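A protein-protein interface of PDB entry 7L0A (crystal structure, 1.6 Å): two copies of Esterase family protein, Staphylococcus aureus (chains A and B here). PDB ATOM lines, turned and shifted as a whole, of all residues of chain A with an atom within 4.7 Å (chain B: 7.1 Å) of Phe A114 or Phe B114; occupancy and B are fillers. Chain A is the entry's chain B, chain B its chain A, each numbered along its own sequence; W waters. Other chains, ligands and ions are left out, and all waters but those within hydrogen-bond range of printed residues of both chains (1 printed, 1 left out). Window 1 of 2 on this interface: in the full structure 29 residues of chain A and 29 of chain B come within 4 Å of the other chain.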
ATOM      1  N   ILE A  12       3.166  -8.789 -12.711  1.00  0.00           N
ATOM      2  CA  ILE A  12       2.268  -7.743 -12.229  1.00  0.00           C
ATOM      3  C   ILE A  12       3.055  -6.672 -11.500  1.00  0.00           C
ATOM      4  O   ILE A  12       3.866  -6.979 -10.622  1.00  0.00           O
ATOM      5  CB  ILE A  12       1.178  -8.354 -11.321  1.00  0.00           C
ATOM      6  CG1 ILE A  12       0.478  -9.506 -12.039  1.00  0.00           C
ATOM      7  CG2 ILE A  12       0.265  -7.266 -10.812  1.00  0.00           C
ATOM      8  CD1 ILE A  12      -0.590 -10.189 -11.213  1.00  0.00           C
ATOM      9  N   LEU A  14       2.107  -3.311  -9.149  1.00  0.00           N
ATOM     10  CA  LEU A  14       0.993  -2.697  -8.444  1.00  0.00           C
ATOM     11  C   LEU A  14       1.474  -1.510  -7.623  1.00  0.00           C
ATOM     12  O   LEU A  14       2.419  -1.637  -6.845  1.00  0.00           O
ATOM     13  CB  LEU A  14       0.320  -3.755  -7.539  1.00  0.00           C
ATOM     14  CG  LEU A  14      -0.974  -3.462  -6.790  1.00  0.00           C
ATOM     15  CD1 LEU A  14      -1.718  -4.783  -6.597  1.00  0.00           C
ATOM     16  CD2 LEU A  14      -0.723  -2.775  -5.451  1.00  0.00           C
ATOM     17  N   VAL A  29       4.397  -8.628  -8.252  1.00  0.00           N
ATOM     18  CA  VAL A  29       3.772  -9.931  -8.018  1.00  0.00           C
ATOM     19  C   VAL A  29       3.954 -10.741  -9.290  1.00  0.00           C
ATOM     20  O   VAL A  29       3.623 -10.276 -10.385  1.00  0.00           O
ATOM     21  CB  VAL A  29       2.282  -9.785  -7.669  1.00  0.00           C
ATOM     22  CG1 VAL A  29       1.620 -11.133  -7.573  1.00  0.00           C
ATOM     23  CG2 VAL A  29       2.112  -9.004  -6.329  1.00  0.00           C
ATOM     24  N   LEU A  31       2.622 -14.279 -10.762  1.00  0.00           N
ATOM     25  CA  LEU A  31       1.501 -15.161 -10.462  1.00  0.00           C
ATOM     26  C   LEU A  31       1.460 -16.263 -11.490  1.00  0.00           C
ATOM     27  O   LEU A  31       1.127 -15.985 -12.658  1.00  0.00           O
ATOM     28  CB  LEU A  31       0.210 -14.347 -10.505  1.00  0.00           C
ATOM     29  CG  LEU A  31      -1.047 -14.937  -9.916  1.00  0.00           C
ATOM     30  CD1 LEU A  31      -0.918 -15.009  -8.392  1.00  0.00           C
ATOM     31  CD2 LEU A  31      -2.247 -14.105 -10.297  1.00  0.00           C
ATOM     32  N   VAL A 110      -2.460  -8.960  -0.521  1.00  0.00           N
ATOM     33  CA  VAL A 110      -2.325  -9.792  -1.721  1.00  0.00           C
ATOM     34  C   VAL A 110      -3.071 -11.103  -1.558  1.00  0.00           C
ATOM     35  O   VAL A 110      -3.530 -11.678  -2.548  1.00  0.00           O
ATOM     36  CB  VAL A 110      -0.850 -10.033  -2.091  1.00  0.00           C
ATOM     37  CG1 VAL A 110      -0.177  -8.681  -2.402  1.00  0.00           C
ATOM     38  CG2 VAL A 110      -0.075 -10.830  -1.055  1.00  0.00           C
ATOM     39  N   HIS A 111      -3.205 -11.612  -0.330  1.00  0.00           N
ATOM     40  CA  HIS A 111      -3.987 -12.832  -0.132  1.00  0.00           C
ATOM     41  C   HIS A 111      -5.486 -12.567  -0.224  1.00  0.00           C
ATOM     42  O   HIS A 111      -6.235 -13.484  -0.578  1.00  0.00           O
ATOM     43  CB  HIS A 111      -3.663 -13.515   1.186  1.00  0.00           C
ATOM     44  CG  HIS A 111      -2.337 -14.226   1.185  1.00  0.00           C
ATOM     45  ND1 HIS A 111      -1.139 -13.567   1.367  1.00  0.00           N
ATOM     46  CD2 HIS A 111      -2.031 -15.535   1.068  1.00  0.00           C
ATOM     47  CE1 HIS A 111      -0.147 -14.444   1.342  1.00  0.00           C
ATOM     48  NE2 HIS A 111      -0.672 -15.651   1.174  1.00  0.00           N
ATOM     49  N   GLN A 112      -5.935 -11.336   0.001  1.00  0.00           N
ATOM     50  CA  GLN A 112      -7.336 -11.017  -0.254  1.00  0.00           C
ATOM     51  C   GLN A 112      -7.631 -10.862  -1.736  1.00  0.00           C
ATOM     52  O   GLN A 112      -8.656 -11.355  -2.222  1.00  0.00           O
ATOM     53  CB  GLN A 112      -7.767  -9.749   0.489  1.00  0.00           C
ATOM     54  CG  GLN A 112      -7.780  -9.845   2.006  1.00  0.00           C
ATOM     55  CD  GLN A 112      -8.802 -10.829   2.542  1.00  0.00           C
ATOM     56  OE1 GLN A 112      -9.997 -10.572   2.485  1.00  0.00           O
ATOM     57  NE2 GLN A 112      -8.332 -11.949   3.075  1.00  0.00           N
ATOM     58  N   ILE A 113      -6.773 -10.119  -2.461  1.00  0.00           N
ATOM     59  CA  ILE A 113      -7.124  -9.748  -3.835  1.00  0.00           C
ATOM     60  C   ILE A 113      -6.606 -10.697  -4.910  1.00  0.00           C
ATOM     61  O   ILE A 113      -7.033 -10.585  -6.073  1.00  0.00           O
ATOM     62  CB  ILE A 113      -6.673  -8.333  -4.248  1.00  0.00           C
ATOM     63  CG1 ILE A 113      -5.156  -8.141  -4.241  1.00  0.00           C
ATOM     64  CG2 ILE A 113      -7.315  -7.277  -3.381  1.00  0.00           C
ATOM     65  CD1 ILE A 113      -4.697  -6.876  -5.012  1.00  0.00           C
ATOM     66  N   PHE A 114      -5.702 -11.615  -4.574  1.00  0.00           N
ATOM     67  CA  PHE A 114      -5.173 -12.582  -5.524  1.00  0.00           C
ATOM     68  C   PHE A 114      -5.457 -14.024  -5.090  1.00  0.00           C
ATOM     69  O   PHE A 114      -5.728 -14.303  -3.907  1.00  0.00           O
ATOM     70  CB  PHE A 114      -3.650 -12.448  -5.737  1.00  0.00           C
ATOM     71  CG  PHE A 114      -3.220 -11.201  -6.449  1.00  0.00           C
ATOM     72  CD1 PHE A 114      -3.562 -10.994  -7.781  1.00  0.00           C
ATOM     73  CD2 PHE A 114      -2.432 -10.267  -5.816  1.00  0.00           C
ATOM     74  CE1 PHE A 114      -3.146  -9.844  -8.434  1.00  0.00           C
ATOM     75  CE2 PHE A 114      -2.020  -9.130  -6.469  1.00  0.00           C
ATOM     76  CZ  PHE A 114      -2.380  -8.922  -7.783  1.00  0.00           C
ATOM     77  N   PRO A 115      -5.393 -14.981  -6.034  1.00  0.00           N
ATOM     78  CA  PRO A 115      -5.698 -16.400  -5.698  1.00  0.00           C
ATOM     79  C   PRO A 115      -4.518 -17.130  -5.063  1.00  0.00           C
ATOM     80  O   PRO A 115      -3.900 -18.040  -5.643  1.00  0.00           O
ATOM     81  CB  PRO A 115      -6.082 -16.979  -7.068  1.00  0.00           C
ATOM     82  CG  PRO A 115      -5.247 -16.193  -8.034  1.00  0.00           C
ATOM     83  CD  PRO A 115      -5.228 -14.774  -7.481  1.00  0.00           C
ATOM     84  N   LEU A 116      -4.166 -16.697  -3.855  1.00  0.00           N
ATOM     85  CA  LEU A 116      -3.010 -17.184  -3.125  1.00  0.00           C
ATOM     86  C   LEU A 116      -3.500 -18.026  -1.957  1.00  0.00           C
ATOM     87  O   LEU A 116      -4.443 -17.634  -1.258  1.00  0.00           O
ATOM     88  CB  LEU A 116      -2.178 -16.021  -2.596  1.00  0.00           C
ATOM     89  CG  LEU A 116      -1.768 -14.958  -3.613  1.00  0.00           C
ATOM     90  CD1 LEU A 116      -0.929 -13.894  -2.998  1.00  0.00           C
ATOM     91  CD2 LEU A 116      -1.036 -15.661  -4.749  1.00  0.00           C
ATOM     92  N   ILE B  12      -2.544  -1.096 -11.594  1.00  0.00           N
ATOM     93  CA  ILE B  12      -2.003  -2.433 -11.836  1.00  0.00           C
ATOM     94  C   ILE B  12      -1.698  -2.584 -13.319  1.00  0.00           C
ATOM     95  O   ILE B  12      -2.571  -2.385 -14.169  1.00  0.00           O
ATOM     96  CB  ILE B  12      -2.963  -3.529 -11.346  1.00  0.00           C
ATOM     97  CG1 ILE B  12      -3.314  -3.317  -9.871  1.00  0.00           C
ATOM     98  CG2 ILE B  12      -2.350  -4.903 -11.634  1.00  0.00           C
ATOM     99  CD1 ILE B  12      -4.321  -4.349  -9.352  1.00  0.00           C
ATOM    100  N   LEU B  14      -0.477  -5.606 -15.830  1.00  0.00           N
ATOM    101  CA  LEU B  14      -0.401  -7.060 -15.870  1.00  0.00           C
ATOM    102  C   LEU B  14      -0.004  -7.516 -17.266  1.00  0.00           C
ATOM    103  O   LEU B  14      -0.567  -7.072 -18.269  1.00  0.00           O
ATOM    104  CB  LEU B  14      -1.749  -7.647 -15.432  1.00  0.00           C
ATOM    105  CG  LEU B  14      -1.898  -9.148 -15.198  1.00  0.00           C
ATOM    106  CD1 LEU B  14      -3.003  -9.318 -14.144  1.00  0.00           C
ATOM    107  CD2 LEU B  14      -2.233  -9.833 -16.470  1.00  0.00           C
ATOM    108  N   LEU B  27      -2.431  -5.856 -19.897  1.00  0.00           N
ATOM    109  CA  LEU B  27      -3.665  -5.311 -19.380  1.00  0.00           C
ATOM    110  C   LEU B  27      -3.332  -4.209 -18.371  1.00  0.00           C
ATOM    111  O   LEU B  27      -2.343  -4.320 -17.615  1.00  0.00           O
ATOM    112  CB  LEU B  27      -4.524  -6.315 -18.611  1.00  0.00           C
ATOM    113  CG  LEU B  27      -4.788  -7.725 -19.105  1.00  0.00           C
ATOM    114  CD1 LEU B  27      -5.572  -8.451 -17.995  1.00  0.00           C
ATOM    115  CD2 LEU B  27      -5.580  -7.672 -20.377  1.00  0.00           C
ATOM    116  N   VAL B  29      -5.295  -2.461 -15.077  1.00  0.00           N
ATOM    117  CA  VAL B  29      -6.419  -2.659 -14.165  1.00  0.00           C
ATOM    118  C   VAL B  29      -6.267  -1.595 -13.103  1.00  0.00           C
ATOM    119  O   VAL B  29      -5.186  -1.454 -12.534  1.00  0.00           O
ATOM    120  CB  VAL B  29      -6.429  -4.061 -13.536  1.00  0.00           C
ATOM    121  CG1 VAL B  29      -7.514  -4.194 -12.434  1.00  0.00           C
ATOM    122  CG2 VAL B  29      -6.660  -5.138 -14.624  1.00  0.00           C
ATOM    123  N   LEU B  31      -7.994  -0.754  -9.540  1.00  0.00           N
ATOM    124  CA  LEU B  31      -8.755  -1.544  -8.578  1.00  0.00           C
ATOM    125  C   LEU B  31      -8.935  -0.731  -7.295  1.00  0.00           C
ATOM    126  O   LEU B  31      -7.936  -0.482  -6.586  1.00  0.00           O
ATOM    127  CB  LEU B  31      -8.039  -2.836  -8.242  1.00  0.00           C
ATOM    128  CG  LEU B  31      -8.794  -3.848  -7.397  1.00  0.00           C
ATOM    129  CD1 LEU B  31      -9.913  -4.470  -8.240  1.00  0.00           C
ATOM    130  CD2 LEU B  31      -7.827  -4.902  -6.902  1.00  0.00           C
ATOM    131  N   PHE B  37     -10.344  -5.472   1.518  1.00  0.00           N
ATOM    132  CA  PHE B  37      -9.161  -6.072   0.921  1.00  0.00           C
ATOM    133  C   PHE B  37      -7.959  -6.029   1.856  1.00  0.00           C
ATOM    134  O   PHE B  37      -6.943  -6.684   1.588  1.00  0.00           O
ATOM    135  CB  PHE B  37      -8.792  -5.384  -0.410  1.00  0.00           C
ATOM    136  CG  PHE B  37      -9.890  -5.360  -1.455  1.00  0.00           C
ATOM    137  CD1 PHE B  37     -11.035  -6.162  -1.376  1.00  0.00           C
ATOM    138  CD2 PHE B  37      -9.740  -4.542  -2.570  1.00  0.00           C
ATOM    139  CE1 PHE B  37     -12.015  -6.094  -2.367  1.00  0.00           C
ATOM    140  CE2 PHE B  37     -10.707  -4.499  -3.574  1.00  0.00           C
ATOM    141  CZ  PHE B  37     -11.842  -5.285  -3.472  1.00  0.00           C
ATOM    142  N   VAL B  44     -14.057 -10.654   1.001  1.00  0.00           N
ATOM    143  CA  VAL B  44     -13.818  -9.490   0.110  1.00  0.00           C
ATOM    144  C   VAL B  44     -15.154  -9.015  -0.456  1.00  0.00           C
ATOM    145  O   VAL B  44     -15.969  -9.842  -0.739  1.00  0.00           O
ATOM    146  CB  VAL B  44     -12.851  -9.807  -1.035  1.00  0.00           C
ATOM    147  CG1 VAL B  44     -11.479 -10.118  -0.505  1.00  0.00           C
ATOM    148  CG2 VAL B  44     -13.365 -10.911  -1.924  1.00  0.00           C
ATOM    149  N   PRO B  46     -17.020  -7.887  -3.560  1.00  0.00           N
ATOM    150  CA  PRO B  46     -16.743  -7.786  -4.982  1.00  0.00           C
ATOM    151  C   PRO B  46     -17.139  -6.409  -5.538  1.00  0.00           C
ATOM    152  O   PRO B  46     -18.158  -5.949  -5.208  1.00  0.00           O
ATOM    153  CB  PRO B  46     -17.571  -8.889  -5.613  1.00  0.00           C
ATOM    154  CG  PRO B  46     -17.912  -9.786  -4.487  1.00  0.00           C
ATOM    155  CD  PRO B  46     -18.041  -8.889  -3.291  1.00  0.00           C
ATOM    156  N   ILE B  81     -11.067  -2.285 -16.329  1.00  0.00           N
ATOM    157  CA  ILE B  81     -10.220  -3.260 -16.996  1.00  0.00           C
ATOM    158  C   ILE B  81      -9.960  -2.735 -18.387  1.00  0.00           C
ATOM    159  O   ILE B  81     -10.909  -2.517 -19.134  1.00  0.00           O
ATOM    160  CB  ILE B  81     -10.891  -4.639 -17.056  1.00  0.00           C
ATOM    161  CG1 ILE B  81     -11.551  -5.043 -15.756  1.00  0.00           C
ATOM    162  CG2 ILE B  81      -9.902  -5.694 -17.588  1.00  0.00           C
ATOM    163  CD1 ILE B  81     -10.664  -5.128 -14.583  1.00  0.00           C
ATOM    164  N   ASP B 108     -13.151 -13.233 -18.102  1.00  0.00           N
ATOM    165  CA  ASP B 108     -13.141 -14.385 -17.207  1.00  0.00           C
ATOM    166  C   ASP B 108     -11.908 -14.376 -16.309  1.00  0.00           C
ATOM    167  O   ASP B 108     -12.007 -14.621 -15.099  1.00  0.00           O
ATOM    168  CB  ASP B 108     -13.206 -15.683 -18.021  1.00  0.00           C
ATOM    169  CG  ASP B 108     -14.584 -15.940 -18.637  1.00  0.00           C
ATOM    170  OD1 ASP B 108     -15.545 -15.232 -18.292  1.00  0.00           O
ATOM    171  OD2 ASP B 108     -14.704 -16.868 -19.490  1.00  0.00           O
ATOM    172  N   TYR B 109     -10.733 -14.090 -16.876  1.00  0.00           N
ATOM    173  CA  TYR B 109      -9.492 -14.099 -16.115  1.00  0.00           C
ATOM    174  C   TYR B 109      -9.511 -13.079 -14.988  1.00  0.00           C
ATOM    175  O   TYR B 109      -9.179 -13.409 -13.840  1.00  0.00           O
ATOM    176  CB  TYR B 109      -8.339 -13.832 -17.069  1.00  0.00           C
ATOM    177  CG  TYR B 109      -6.960 -13.818 -16.474  1.00  0.00           C
ATOM    178  CD1 TYR B 109      -6.457 -14.913 -15.783  1.00  0.00           C
ATOM    179  CD2 TYR B 109      -6.148 -12.705 -16.619  1.00  0.00           C
ATOM    180  CE1 TYR B 109      -5.179 -14.900 -15.258  1.00  0.00           C
ATOM    181  CE2 TYR B 109      -4.861 -12.688 -16.116  1.00  0.00           C
ATOM    182  CZ  TYR B 109      -4.393 -13.783 -15.426  1.00  0.00           C
ATOM    183  OH  TYR B 109      -3.106 -13.756 -14.914  1.00  0.00           O
ATOM    184  N   VAL B 110      -9.895 -11.829 -15.285  1.00  0.00           N
ATOM    185  CA  VAL B 110      -9.826 -10.823 -14.231  1.00  0.00           C
ATOM    186  C   VAL B 110     -10.900 -11.072 -13.176  1.00  0.00           C
ATOM    187  O   VAL B 110     -10.699 -10.746 -12.004  1.00  0.00           O
ATOM    188  CB  VAL B 110      -9.902  -9.377 -14.773  1.00  0.00           C
ATOM    189  CG1 VAL B 110      -8.698  -9.098 -15.667  1.00  0.00           C
ATOM    190  CG2 VAL B 110     -11.251  -9.109 -15.464  1.00  0.00           C
ATOM    191  N   HIS B 111     -12.056 -11.634 -13.553  1.00  0.00           N
ATOM    192  CA  HIS B 111     -13.051 -11.958 -12.523  1.00  0.00           C
ATOM    193  C   HIS B 111     -12.636 -13.180 -11.702  1.00  0.00           C
ATOM    194  O   HIS B 111     -13.059 -13.295 -10.542  1.00  0.00           O
ATOM    195  CB  HIS B 111     -14.429 -12.155 -13.124  1.00  0.00           C
ATOM    196  CG  HIS B 111     -15.086 -10.889 -13.591  1.00  0.00           C
ATOM    197  ND1 HIS B 111     -14.710 -10.255 -14.757  1.00  0.00           N
ATOM    198  CD2 HIS B 111     -16.047 -10.108 -13.040  1.00  0.00           C
ATOM    199  CE1 HIS B 111     -15.456  -9.179 -14.937  1.00  0.00           C
ATOM    200  NE2 HIS B 111     -16.250  -9.051 -13.893  1.00  0.00           N
ATOM    201  N   GLN B 112     -11.777 -14.051 -12.235  1.00  0.00           N
ATOM    202  CA  GLN B 112     -11.252 -15.141 -11.422  1.00  0.00           C
ATOM    203  C   GLN B 112     -10.179 -14.664 -10.457  1.00  0.00           C
ATOM    204  O   GLN B 112     -10.226 -15.019  -9.265  1.00  0.00           O
ATOM    205  CB  GLN B 112     -10.697 -16.269 -12.306  1.00  0.00           C
ATOM    206  CG  GLN B 112     -11.766 -17.058 -13.040  1.00  0.00           C
ATOM    207  CD  GLN B 112     -12.724 -17.779 -12.110  1.00  0.00           C
ATOM    208  OE1 GLN B 112     -12.356 -18.731 -11.438  1.00  0.00           O
ATOM    209  NE2 GLN B 112     -13.977 -17.340 -12.095  1.00  0.00           N
ATOM    210  N   ILE B 113      -9.255 -13.810 -10.905  1.00  0.00           N
ATOM    211  CA  ILE B 113      -8.093 -13.540 -10.073  1.00  0.00           C
ATOM    212  C   ILE B 113      -8.227 -12.281  -9.224  1.00  0.00           C
ATOM    213  O   ILE B 113      -7.397 -12.061  -8.331  1.00  0.00           O
ATOM    214  CB  ILE B 113      -6.781 -13.438 -10.872  1.00  0.00           C
ATOM    215  CG1 ILE B 113      -6.740 -12.228 -11.793  1.00  0.00           C
ATOM    216  CG2 ILE B 113      -6.541 -14.748 -11.638  1.00  0.00           C
ATOM    217  CD1 ILE B 113      -5.340 -11.954 -12.338  1.00  0.00           C
ATOM    218  N   PHE B 114      -9.215 -11.439  -9.482  1.00  0.00           N
ATOM    219  CA  PHE B 114      -9.441 -10.207  -8.747  1.00  0.00           C
ATOM    220  C   PHE B 114     -10.825 -10.207  -8.094  1.00  0.00           C
ATOM    221  O   PHE B 114     -11.737 -10.916  -8.537  1.00  0.00           O
ATOM    222  CB  PHE B 114      -9.354  -8.972  -9.645  1.00  0.00           C
ATOM    223  CG  PHE B 114      -7.979  -8.624 -10.089  1.00  0.00           C
ATOM    224  CD1 PHE B 114      -7.022  -8.247  -9.183  1.00  0.00           C
ATOM    225  CD2 PHE B 114      -7.659  -8.628 -11.436  1.00  0.00           C
ATOM    226  CE1 PHE B 114      -5.756  -7.885  -9.600  1.00  0.00           C
ATOM    227  CE2 PHE B 114      -6.385  -8.271 -11.867  1.00  0.00           C
ATOM    228  CZ  PHE B 114      -5.435  -7.901 -10.933  1.00  0.00           C
ATOM    229  N   PRO B 115     -11.030  -9.374  -7.029  1.00  0.00           N
ATOM    230  CA  PRO B 115     -12.336  -9.266  -6.335  1.00  0.00           C
ATOM    231  C   PRO B 115     -13.367  -8.418  -7.075  1.00  0.00           C
ATOM    232  O   PRO B 115     -13.759  -7.316  -6.660  1.00  0.00           O
ATOM    233  CB  PRO B 115     -11.935  -8.656  -4.982  1.00  0.00           C
ATOM    234  CG  PRO B 115     -10.727  -7.785  -5.356  1.00  0.00           C
ATOM    235  CD  PRO B 115      -9.962  -8.599  -6.351  1.00  0.00           C
ATOM    236  N   LEU B 116     -13.820  -8.962  -8.194  1.00  0.00           N
ATOM    237  CA  LEU B 116     -14.746  -8.299  -9.104  1.00  0.00           C
ATOM    238  C   LEU B 116     -16.089  -8.995  -9.089  1.00  0.00           C
ATOM    239  O   LEU B 116     -16.156 -10.223  -9.164  1.00  0.00           O
ATOM    240  CB  LEU B 116     -14.200  -8.308 -10.526  1.00  0.00           C
ATOM    241  CG  LEU B 116     -12.792  -7.737 -10.665  1.00  0.00           C
ATOM    242  CD1 LEU B 116     -12.363  -7.834 -12.130  1.00  0.00           C
ATOM    243  CD2 LEU B 116     -12.686  -6.337 -10.170  1.00  0.00           C
ATOM    244  N   SER B 117     -17.154  -8.212  -8.977  1.00  0.00           N
ATOM    245  CA  SER B 117     -18.482  -8.781  -8.974  1.00  0.00           C
ATOM    246  C   SER B 117     -18.738  -9.523 -10.264  1.00  0.00           C
ATOM    247  O   SER B 117     -18.392  -9.039 -11.352  1.00  0.00           O
ATOM    248  CB  SER B 117     -19.537  -7.692  -8.809  1.00  0.00           C
ATOM    249  OG  SER B 117     -20.830  -8.300  -8.847  1.00  0.00           O
ATOM    250  N   LYS B 118     -19.370 -10.686 -10.143  1.00  0.00           N
ATOM    251  CA  LYS B 118     -19.773 -11.485 -11.294  1.00  0.00           C
ATOM    252  C   LYS B 118     -21.222 -11.256 -11.690  1.00  0.00           C
ATOM    253  O   LYS B 118     -21.688 -11.846 -12.683  1.00  0.00           O
ATOM    254  CB  LYS B 118     -19.526 -12.963 -10.996  1.00  0.00           C
ATOM    255  CG  LYS B 118     -18.016 -13.276 -10.869  1.00  0.00           C
ATOM    256  CD  LYS B 118     -17.741 -14.615 -10.201  1.00  0.00           C
ATOM    257  CE  LYS B 118     -16.243 -14.833 -10.053  1.00  0.00           C
ATOM    258  NZ  LYS B 118     -15.915 -16.204  -9.558  1.00  0.00           N
HETATM  259  O   HOH W   1      -1.705 -15.938 -13.659  1.00  0.00           O
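Of the 11 printed residues of chain A, 6 touch a printed residue of chain B.
Among the printed residues, no Asp or Glu carboxylate lies within 4 Å of a Lys or Arg side-chain nitrogen of the other chain.
The backbone carbonyl oxygen of Val B29 lies within hydrogen-bond range of the backbone NH of Ile B12.
The backbone carbonyl oxygen (O) of Leu B14 sits at hydrogen-bond distance from the backbone NH (N) of Leu B27 (2.8 Å).
The backbone NH of Ile A12 sits at hydrogen-bond distance from the backbone carbonyl oxygen of Val A29 (2.8 Å).
O of Ile B113 lies close to O of Ile A113.
Phe A114 touches just these residues of chain B: Ile B113 and Phe B114.
Of the printed residues of chain A, Phe B114 touches Ile A113 (3.6 Å) and Phe A114 (3.5 Å).
Printed residues of chain A within 4 Å of Phe B37: Gln A112 and Ile A113.
Printed residues of chain A within 4 Å of Ile B12: Ile A12 and Leu A14.
Printed residues of chain B within 4 Å of Pro A115: Ile B113 (3.6 Å).
Of the printed residues of chain A, Val B44 touches Gln A112.
Of the printed residues of chain A, Pro B115 touches Ile A113 (3.5 Å).
Asp B108 touches none of the printed residues of chain A.
Ser B117 touches none of the printed residues of chain A.
The nearest residue of chain B that does not touch Phe A114 is Ile B12 (5.2 Å).
The nearest printed residue of chain A that does not touch Phe B114 is Ile A12 (5.4 Å).
Ile A12 touches its own counterpart, Ile B12.
Ile A12 touches Leu B14, and with the chains exchanged Leu A14 touches Ile B12.
Ile A113 touches Phe B114, and with the chains exchanged Phe A114 touches Ile B113.
Ile A113 touches Pro B115, and with the chains exchanged Pro A115 touches Ile B113.
11 positions are printed for both chains.
Water W1 bridges the side-chain hydroxyl (OH) of Tyr B109 (2.9 Å) and the backbone carbonyl oxygen (O) of Leu A31 (3.0 Å).
Among the printed residues, merely in contact across the chains: Gln A112 with Phe B37 (3.3 Å), Gln A112 with Val B44 (3.4 Å), Phe A114 with Phe B114 (3.5 Å), Ile A113 with Pro B115 (3.5 Å), Pro A115 with Ile B113 (3.6 Å), Ile A113 with Phe B114 (3.6 Å), Phe A114 with Ile B113 (3.6 Å), Ile A12 with Ile B12 (3.6 Å), Ile A113 with Phe B37 (3.7 Å), Leu A14 with Ile B12 (3.8 Å) and Ile A12 with Leu B14 (3.9 Å).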
